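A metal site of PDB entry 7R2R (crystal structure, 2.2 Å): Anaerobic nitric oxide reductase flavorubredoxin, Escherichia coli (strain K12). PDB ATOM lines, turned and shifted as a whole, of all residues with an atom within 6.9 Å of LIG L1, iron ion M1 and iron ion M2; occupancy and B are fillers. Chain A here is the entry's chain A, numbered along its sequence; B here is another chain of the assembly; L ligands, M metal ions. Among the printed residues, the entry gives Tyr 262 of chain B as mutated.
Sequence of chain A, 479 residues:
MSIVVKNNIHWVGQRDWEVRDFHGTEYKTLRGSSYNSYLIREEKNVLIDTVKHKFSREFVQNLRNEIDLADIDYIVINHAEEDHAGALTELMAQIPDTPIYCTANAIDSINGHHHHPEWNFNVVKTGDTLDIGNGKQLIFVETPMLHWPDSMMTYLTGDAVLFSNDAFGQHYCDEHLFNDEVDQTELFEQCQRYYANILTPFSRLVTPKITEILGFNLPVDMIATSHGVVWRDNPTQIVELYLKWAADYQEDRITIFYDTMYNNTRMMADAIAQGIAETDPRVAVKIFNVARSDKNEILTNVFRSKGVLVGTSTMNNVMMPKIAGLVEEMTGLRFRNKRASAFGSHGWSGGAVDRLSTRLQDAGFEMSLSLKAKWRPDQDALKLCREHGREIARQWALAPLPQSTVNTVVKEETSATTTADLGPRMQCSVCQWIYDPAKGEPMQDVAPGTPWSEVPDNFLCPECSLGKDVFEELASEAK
Four residues have an atom within 4 Å of iron ion M2: His 79, Glu 81, His 147 and Asp 166.
Within 4 Å of iron ion M1: Asp 83, His 84, Asp 166 and His 227.
Iron ion M2 is bound by the side-chain carboxylate of Glu 81 (2.0 Å), the side-chain carboxylate of Asp 166 (2.0 Å), a ring nitrogen (NE2) of His 147 (2.1 Å), an oxygen (O1) of LG2 L2 (2.2 Å) and a ring nitrogen (NE2) of His 79 (2.4 Å).
The side-chain carboxylate (OD1) of Asp 166 lies close to the side-chain hydroxyl (OH) of Tyr 194 (3.5 Å). The backbone NH (N) of Asp 166 is in hydrogen-bond range of the side-chain hydroxyl (OG) of Ser 226. A ring nitrogen (ND1) of His 147 sits close to the indole nitrogen (NE1) of Trp 148. The side-chain hydroxyl (OG) of Ser 151 sits at hydrogen-bond distance from the backbone NH (N) of His 147 (3.5 Å). The side-chain hydroxyl of Ser 226 sits close to a ring nitrogen (NE2) of His 84. O of Ser 34 is in hydrogen-bond range of ND1 of His 227, 2.8 Å away.
O1 of LG2 L2 binds iron ion M1 (2.1 Å). NE2 of His 84 binds iron ion M1 (2.1 Å). Iron ion M1 is bound by OD2 of Asp 83 (2.1 Å). A ring nitrogen (NE2) of His 227 binds iron ion M1 (2.2 Å). Iron ion M1 is bound by an oxygen (O2) of LIG L1 (2.4 Å). OD1 of Asp 166 is bound to iron ion M1, at 2.4 Å.
The side-chain hydroxyl (OH) of Tyr 194 is in hydrogen-bond range of an oxygen (O1) of LIG L1. The backbone NH (N) of Tyr 262 of chain B lies within hydrogen-bond range of an oxygen (O9) of LG3 L3, at 2.9 Å.
The nearest printed residue that does not touch LIG L1 is Glu 81 (4.2 Å).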
ATOM      1  N   PHE A  22       3.396 -16.337   6.777  1.00  0.00           N
ATOM      2  CA  PHE A  22       3.833 -15.028   7.257  1.00  0.00           C
ATOM      3  C   PHE A  22       3.742 -14.000   6.140  1.00  0.00           C
ATOM      4  O   PHE A  22       3.843 -14.348   4.964  1.00  0.00           O
ATOM      5  CB  PHE A  22       5.256 -15.089   7.809  1.00  0.00           C
ATOM      6  CG  PHE A  22       5.328 -15.168   9.307  1.00  0.00           C
ATOM      7  CD1 PHE A  22       5.349 -16.378   9.963  1.00  0.00           C
ATOM      8  CD2 PHE A  22       5.384 -14.002  10.065  1.00  0.00           C
ATOM      9  CE1 PHE A  22       5.420 -16.451  11.345  1.00  0.00           C
ATOM     10  CE2 PHE A  22       5.452 -14.061  11.448  1.00  0.00           C
ATOM     11  CZ  PHE A  22       5.462 -15.288  12.089  1.00  0.00           C
ATOM     12  N   HIS A  23       3.557 -12.732   6.518  1.00  0.00           N
ATOM     13  CA  HIS A  23       3.380 -11.643   5.553  1.00  0.00           C
ATOM     14  C   HIS A  23       2.255 -11.974   4.588  1.00  0.00           C
ATOM     15  O   HIS A  23       2.435 -11.902   3.367  1.00  0.00           O
ATOM     16  CB  HIS A  23       4.676 -11.364   4.790  1.00  0.00           C
ATOM     17  CG  HIS A  23       5.835 -11.044   5.678  1.00  0.00           C
ATOM     18  ND1 HIS A  23       7.148 -11.074   5.232  1.00  0.00           N
ATOM     19  CD2 HIS A  23       5.891 -10.682   6.980  1.00  0.00           C
ATOM     20  CE1 HIS A  23       7.951 -10.738   6.226  1.00  0.00           C
ATOM     21  NE2 HIS A  23       7.220 -10.506   7.294  1.00  0.00           N
ATOM     22  N   SER A  34       8.761 -19.097  16.469  1.00  0.00           N
ATOM     23  CA  SER A  34       8.585 -18.726  17.865  1.00  0.00           C
ATOM     24  C   SER A  34       8.622 -17.215  18.011  1.00  0.00           C
ATOM     25  O   SER A  34       9.232 -16.508  17.199  1.00  0.00           O
ATOM     26  CB  SER A  34       9.667 -19.373  18.737  1.00  0.00           C
ATOM     27  OG  SER A  34      10.942 -18.817  18.454  1.00  0.00           O
ATOM     28  N   TYR A  35       7.959 -16.711  19.045  1.00  0.00           N
ATOM     29  CA  TYR A  35       7.947 -15.284  19.330  1.00  0.00           C
ATOM     30  C   TYR A  35       8.524 -15.061  20.712  1.00  0.00           C
ATOM     31  O   TYR A  35       7.827 -15.232  21.718  1.00  0.00           O
ATOM     32  CB  TYR A  35       6.534 -14.726  19.214  1.00  0.00           C
ATOM     33  CG  TYR A  35       5.766 -15.292  18.037  1.00  0.00           C
ATOM     34  CD1 TYR A  35       6.092 -14.930  16.741  1.00  0.00           C
ATOM     35  CD2 TYR A  35       4.744 -16.207  18.225  1.00  0.00           C
ATOM     36  CE1 TYR A  35       5.408 -15.460  15.659  1.00  0.00           C
ATOM     37  CE2 TYR A  35       4.051 -16.733  17.166  1.00  0.00           C
ATOM     38  CZ  TYR A  35       4.381 -16.356  15.877  1.00  0.00           C
ATOM     39  OH  TYR A  35       3.695 -16.887  14.813  1.00  0.00           O
ATOM     40  N   HIS A  79      10.554  -3.387  18.412  1.00  0.00           N
ATOM     41  CA  HIS A  79       9.944  -3.526  17.107  1.00  0.00           C
ATOM     42  C   HIS A  79       8.438  -3.706  17.255  1.00  0.00           C
ATOM     43  O   HIS A  79       7.993  -4.570  18.011  1.00  0.00           O
ATOM     44  CB  HIS A  79      10.570  -4.720  16.371  1.00  0.00           C
ATOM     45  CG  HIS A  79      10.139  -4.857  14.938  1.00  0.00           C
ATOM     46  ND1 HIS A  79       9.973  -3.786  14.095  1.00  0.00           N
ATOM     47  CD2 HIS A  79       9.854  -5.959  14.202  1.00  0.00           C
ATOM     48  CE1 HIS A  79       9.597  -4.205  12.905  1.00  0.00           C
ATOM     49  NE2 HIS A  79       9.519  -5.531  12.943  1.00  0.00           N
ATOM     50  N   GLU A  81       6.057  -4.564  15.046  1.00  0.00           N
ATOM     51  CA  GLU A  81       5.339  -5.429  14.121  1.00  0.00           C
ATOM     52  C   GLU A  81       4.461  -6.370  14.921  1.00  0.00           C
ATOM     53  O   GLU A  81       4.801  -6.762  16.038  1.00  0.00           O
ATOM     54  CB  GLU A  81       6.311  -6.203  13.223  1.00  0.00           C
ATOM     55  CG  GLU A  81       5.652  -6.897  12.044  1.00  0.00           C
ATOM     56  CD  GLU A  81       6.644  -7.355  10.992  1.00  0.00           C
ATOM     57  OE1 GLU A  81       7.858  -7.125  11.156  1.00  0.00           O
ATOM     58  OE2 GLU A  81       6.214  -7.954   9.979  1.00  0.00           O
ATOM     59  N   ASP A  83       3.804  -9.342  15.229  1.00  0.00           N
ATOM     60  CA  ASP A  83       4.289 -10.603  15.789  1.00  0.00           C
ATOM     61  C   ASP A  83       5.127 -10.395  17.046  1.00  0.00           C
ATOM     62  O   ASP A  83       5.605 -11.361  17.646  1.00  0.00           O
ATOM     63  CB  ASP A  83       5.100 -11.370  14.736  1.00  0.00           C
ATOM     64  CG  ASP A  83       6.286 -10.583  14.227  1.00  0.00           C
ATOM     65  OD1 ASP A  83       6.180  -9.333  14.147  1.00  0.00           O
ATOM     66  OD2 ASP A  83       7.322 -11.205  13.903  1.00  0.00           O
ATOM     67  N   HIS A  84       5.314  -9.146  17.448  1.00  0.00           N
ATOM     68  CA  HIS A  84       6.094  -8.840  18.647  1.00  0.00           C
ATOM     69  C   HIS A  84       5.370  -7.865  19.570  1.00  0.00           C
ATOM     70  O   HIS A  84       5.611  -7.841  20.771  1.00  0.00           O
ATOM     71  CB  HIS A  84       7.462  -8.280  18.266  1.00  0.00           C
ATOM     72  CG  HIS A  84       8.207  -9.116  17.281  1.00  0.00           C
ATOM     73  ND1 HIS A  84       8.577 -10.416  17.531  1.00  0.00           N
ATOM     74  CD2 HIS A  84       8.645  -8.832  16.029  1.00  0.00           C
ATOM     75  CE1 HIS A  84       9.209 -10.904  16.483  1.00  0.00           C
ATOM     76  NE2 HIS A  84       9.270  -9.967  15.560  1.00  0.00           N
ATOM     77  N   HIS A 147      14.448  -4.335  10.217  1.00  0.00           N
ATOM     78  CA  HIS A 147      14.054  -4.080   8.831  1.00  0.00           C
ATOM     79  C   HIS A 147      13.013  -2.968   8.719  1.00  0.00           C
ATOM     80  O   HIS A 147      12.510  -2.673   7.644  1.00  0.00           O
ATOM     81  CB  HIS A 147      13.523  -5.366   8.183  1.00  0.00           C
ATOM     82  CG  HIS A 147      12.297  -5.901   8.847  1.00  0.00           C
ATOM     83  ND1 HIS A 147      11.017  -5.581   8.432  1.00  0.00           N
ATOM     84  CD2 HIS A 147      12.143  -6.735   9.907  1.00  0.00           C
ATOM     85  CE1 HIS A 147      10.142  -6.201   9.199  1.00  0.00           C
ATOM     86  NE2 HIS A 147      10.794  -6.896  10.105  1.00  0.00           N
ATOM     87  N   TRP A 148      12.689  -2.349   9.858  1.00  0.00           N
ATOM     88  CA  TRP A 148      11.694  -1.276   9.895  1.00  0.00           C
ATOM     89  C   TRP A 148      12.316   0.015  10.403  1.00  0.00           C
ATOM     90  O   TRP A 148      13.380   0.000  11.030  1.00  0.00           O
ATOM     91  CB  TRP A 148      10.511  -1.674  10.780  1.00  0.00           C
ATOM     92  CG  TRP A 148       9.388  -2.364  10.055  1.00  0.00           C
ATOM     93  CD1 TRP A 148       9.445  -2.936   8.821  1.00  0.00           C
ATOM     94  CD2 TRP A 148       8.043  -2.545  10.515  1.00  0.00           C
ATOM     95  NE1 TRP A 148       8.226  -3.471   8.487  1.00  0.00           N
ATOM     96  CE2 TRP A 148       7.342  -3.242   9.512  1.00  0.00           C
ATOM     97  CE3 TRP A 148       7.358  -2.183  11.687  1.00  0.00           C
ATOM     98  CZ2 TRP A 148       5.996  -3.581   9.638  1.00  0.00           C
ATOM     99  CZ3 TRP A 148       6.029  -2.519  11.810  1.00  0.00           C
ATOM    100  CH2 TRP A 148       5.360  -3.215  10.787  1.00  0.00           C
ATOM    101  N   SER A 151      12.865  -0.077  14.233  1.00  0.00           N
ATOM    102  CA  SER A 151      13.679  -1.154  14.780  1.00  0.00           C
ATOM    103  C   SER A 151      14.845  -0.663  15.629  1.00  0.00           C
ATOM    104  O   SER A 151      15.498   0.335  15.301  1.00  0.00           O
ATOM    105  CB  SER A 151      14.207  -2.039  13.652  1.00  0.00           C
ATOM    106  OG  SER A 151      13.137  -2.592  12.904  1.00  0.00           O
ATOM    107  N   ASN A 165      16.088  -8.569  18.606  1.00  0.00           N
ATOM    108  CA  ASN A 165      14.780  -8.710  17.970  1.00  0.00           C
ATOM    109  C   ASN A 165      14.868  -9.550  16.696  1.00  0.00           C
ATOM    110  O   ASN A 165      15.373 -10.664  16.727  1.00  0.00           O
ATOM    111  CB  ASN A 165      14.178  -7.330  17.685  1.00  0.00           C
ATOM    112  CG  ASN A 165      12.676  -7.383  17.469  1.00  0.00           C
ATOM    113  OD1 ASN A 165      12.206  -7.426  16.336  1.00  0.00           O
ATOM    114  ND2 ASN A 165      11.915  -7.376  18.568  1.00  0.00           N
ATOM    115  N   ASP A 166      14.389  -9.008  15.578  1.00  0.00           N
ATOM    116  CA  ASP A 166      14.355  -9.738  14.308  1.00  0.00           C
ATOM    117  C   ASP A 166      15.742 -10.118  13.792  1.00  0.00           C
ATOM    118  O   ASP A 166      15.918 -11.181  13.195  1.00  0.00           O
ATOM    119  CB  ASP A 166      13.632  -8.919  13.234  1.00  0.00           C
ATOM    120  CG  ASP A 166      12.129  -9.101  13.276  1.00  0.00           C
ATOM    121  OD1 ASP A 166      11.654 -10.040  13.947  1.00  0.00           O
ATOM    122  OD2 ASP A 166      11.421  -8.315  12.615  1.00  0.00           O
ATOM    123  N   HIS A 171      12.882 -18.359  11.641  1.00  0.00           N
ATOM    124  CA  HIS A 171      11.624 -19.055  11.903  1.00  0.00           C
ATOM    125  C   HIS A 171      11.872 -20.552  12.069  1.00  0.00           C
ATOM    126  O   HIS A 171      11.801 -21.320  11.106  1.00  0.00           O
ATOM    127  CB  HIS A 171      10.614 -18.793  10.794  1.00  0.00           C
ATOM    128  CG  HIS A 171      10.199 -17.351  10.695  1.00  0.00           C
ATOM    129  ND1 HIS A 171       9.527 -16.702  11.698  1.00  0.00           N
ATOM    130  CD2 HIS A 171      10.369 -16.444   9.708  1.00  0.00           C
ATOM    131  CE1 HIS A 171       9.293 -15.453  11.345  1.00  0.00           C
ATOM    132  NE2 HIS A 171       9.792 -15.267  10.134  1.00  0.00           N
ATOM    133  N   TYR A 194      15.682 -16.755   6.032  1.00  0.00           N
ATOM    134  CA  TYR A 194      15.165 -15.538   6.650  1.00  0.00           C
ATOM    135  C   TYR A 194      15.819 -14.289   6.085  1.00  0.00           C
ATOM    136  O   TYR A 194      15.141 -13.329   5.739  1.00  0.00           O
ATOM    137  CB  TYR A 194      15.359 -15.604   8.165  1.00  0.00           C
ATOM    138  CG  TYR A 194      14.726 -14.449   8.915  1.00  0.00           C
ATOM    139  CD1 TYR A 194      15.465 -13.318   9.244  1.00  0.00           C
ATOM    140  CD2 TYR A 194      13.388 -14.494   9.299  1.00  0.00           C
ATOM    141  CE1 TYR A 194      14.890 -12.262   9.924  1.00  0.00           C
ATOM    142  CE2 TYR A 194      12.810 -13.446   9.983  1.00  0.00           C
ATOM    143  CZ  TYR A 194      13.567 -12.332  10.296  1.00  0.00           C
ATOM    144  OH  TYR A 194      12.989 -11.284  10.981  1.00  0.00           O
ATOM    145  N   ILE A 198      13.986 -11.413   3.526  1.00  0.00           N
ATOM    146  CA  ILE A 198      13.622 -10.258   4.346  1.00  0.00           C
ATOM    147  C   ILE A 198      14.654  -9.124   4.311  1.00  0.00           C
ATOM    148  O   ILE A 198      14.308  -7.978   4.064  1.00  0.00           O
ATOM    149  CB  ILE A 198      13.387 -10.652   5.815  1.00  0.00           C
ATOM    150  CG1 ILE A 198      12.380 -11.806   5.916  1.00  0.00           C
ATOM    151  CG2 ILE A 198      12.930  -9.460   6.637  1.00  0.00           C
ATOM    152  CD1 ILE A 198      11.066 -11.511   5.249  1.00  0.00           C
ATOM    153  N   SER A 226      14.194 -12.385  18.583  1.00  0.00           N
ATOM    154  CA  SER A 226      12.753 -12.437  18.784  1.00  0.00           C
ATOM    155  C   SER A 226      12.152 -13.656  18.079  1.00  0.00           C
ATOM    156  O   SER A 226      10.978 -13.974  18.271  1.00  0.00           O
ATOM    157  CB  SER A 226      12.092 -11.154  18.273  1.00  0.00           C
ATOM    158  OG  SER A 226      12.257 -11.026  16.868  1.00  0.00           O
ATOM    159  N   HIS A 227      12.975 -14.331  17.275  1.00  0.00           N
ATOM    160  CA  HIS A 227      12.536 -15.519  16.541  1.00  0.00           C
ATOM    161  C   HIS A 227      13.557 -16.651  16.649  1.00  0.00           C
ATOM    162  O   HIS A 227      14.718 -16.473  16.294  1.00  0.00           O
ATOM    163  CB  HIS A 227      12.284 -15.199  15.068  1.00  0.00           C
ATOM    164  CG  HIS A 227      11.104 -14.329  14.826  1.00  0.00           C
ATOM    165  ND1 HIS A 227       9.817 -14.700  15.144  1.00  0.00           N
ATOM    166  CD2 HIS A 227      10.999 -13.092  14.267  1.00  0.00           C
ATOM    167  CE1 HIS A 227       8.979 -13.748  14.807  1.00  0.00           C
ATOM    168  NE2 HIS A 227       9.668 -12.754  14.267  1.00  0.00           N
ATOM    169  N   TYR B 262      -1.545  -7.970   7.118  1.00  0.00           N
ATOM    170  CA  TYR B 262      -2.063  -7.797   8.472  1.00  0.00           C
ATOM    171  C   TYR B 262      -3.488  -7.256   8.487  1.00  0.00           C
ATOM    172  O   TYR B 262      -3.906  -6.636   9.463  1.00  0.00           O
ATOM    173  CB  TYR B 262      -1.142  -6.874   9.276  1.00  0.00           C
ATOM    174  CG  TYR B 262       0.261  -7.406   9.427  1.00  0.00           C
ATOM    175  CD1 TYR B 262       0.510  -8.548  10.182  1.00  0.00           C
ATOM    176  CD2 TYR B 262       1.334  -6.778   8.804  1.00  0.00           C
ATOM    177  CE1 TYR B 262       1.786  -9.036  10.327  1.00  0.00           C
ATOM    178  CE2 TYR B 262       2.629  -7.276   8.944  1.00  0.00           C
ATOM    179  CZ  TYR B 262       2.845  -8.403   9.701  1.00  0.00           C
ATOM    180  OH  TYR B 262       4.118  -8.900   9.850  1.00  0.00           O
HETATM  181  O1  LIG L   1      10.222 -10.522  10.373  1.00  0.00           O
HETATM  182  O2  LIG L   1      10.062 -11.187  11.363  1.00  0.00           O
HETATM  183  O1  LG2 L   2       8.584  -8.837  13.165  1.00  0.00           O
HETATM  184  N1  LG3 L   3       5.558   0.206   4.377  1.00  0.00           N
HETATM  185  C1  LG3 L   3       5.975   1.198   3.510  1.00  0.00           C
HETATM  186  O1  LG3 L   3       5.462   2.314   3.560  1.00  0.00           O
HETATM  187  N2  LG3 L   3       6.975   0.947   2.586  1.00  0.00           N
HETATM  188  C2  LG3 L   3       7.549  -0.307   2.527  1.00  0.00           C
HETATM  189  O2  LG3 L   3       8.447  -0.521   1.704  1.00  0.00           O
HETATM  190  C3  LG3 L   3       7.139  -1.305   3.389  1.00  0.00           C
HETATM  191  N3  LG3 L   3       7.720  -2.557   3.337  1.00  0.00           N
HETATM  192  C4  LG3 L   3       7.297  -3.551   4.198  1.00  0.00           C
HETATM  193  C5  LG3 L   3       7.884  -4.809   4.140  1.00  0.00           C
HETATM  194  C6  LG3 L   3       7.467  -5.809   4.995  1.00  0.00           C
HETATM  195  C7  LG3 L   3       8.112  -7.169   4.926  1.00  0.00           C
HETATM  196  C8  LG3 L   3       6.470  -5.564   5.931  1.00  0.00           C
HETATM  197  C9  LG3 L   3       6.014  -6.635   6.868  1.00  0.00           C
HETATM  198  C10 LG3 L   3       5.883  -4.306   5.988  1.00  0.00           C
HETATM  199  C11 LG3 L   3       6.290  -3.294   5.127  1.00  0.00           C
HETATM  200  N4  LG3 L   3       5.709  -2.042   5.179  1.00  0.00           N
HETATM  201  C12 LG3 L   3       6.132  -1.048   4.318  1.00  0.00           C
HETATM  202  C13 LG3 L   3       4.627  -1.740   6.177  1.00  0.00           C
HETATM  203  C14 LG3 L   3       3.238  -2.138   5.675  1.00  0.00           C
HETATM  204  O3  LG3 L   3       2.958  -1.503   4.450  1.00  0.00           O
HETATM  205  C15 LG3 L   3       2.191  -1.758   6.725  1.00  0.00           C
HETATM  206  O4  LG3 L   3       2.331  -2.608   7.845  1.00  0.00           O
HETATM  207  C16 LG3 L   3       0.757  -1.867   6.187  1.00  0.00           C
HETATM  208  O5  LG3 L   3      -0.074  -1.024   6.939  1.00  0.00           O
HETATM  209  C17 LG3 L   3       0.225  -3.290   6.264  1.00  0.00           C
HETATM  210  O6  LG3 L   3      -0.677  -3.515   5.207  1.00  0.00           O
HETATM  211  P1  LG3 L   3      -1.639  -4.804   5.169  1.00  0.00           P
HETATM  212  O7  LG3 L   3      -2.885  -4.446   4.405  1.00  0.00           O
HETATM  213  O8  LG3 L   3      -0.921  -5.945   4.501  1.00  0.00           O
HETATM  214  O9  LG3 L   3      -2.028  -5.186   6.578  1.00  0.00           O
HETATM  215 FE    FE M   1       9.340 -10.712  13.601  1.00  0.00          FE
HETATM  216 FE    FE M   2       9.726  -7.630  11.720  1.00  0.00          FE
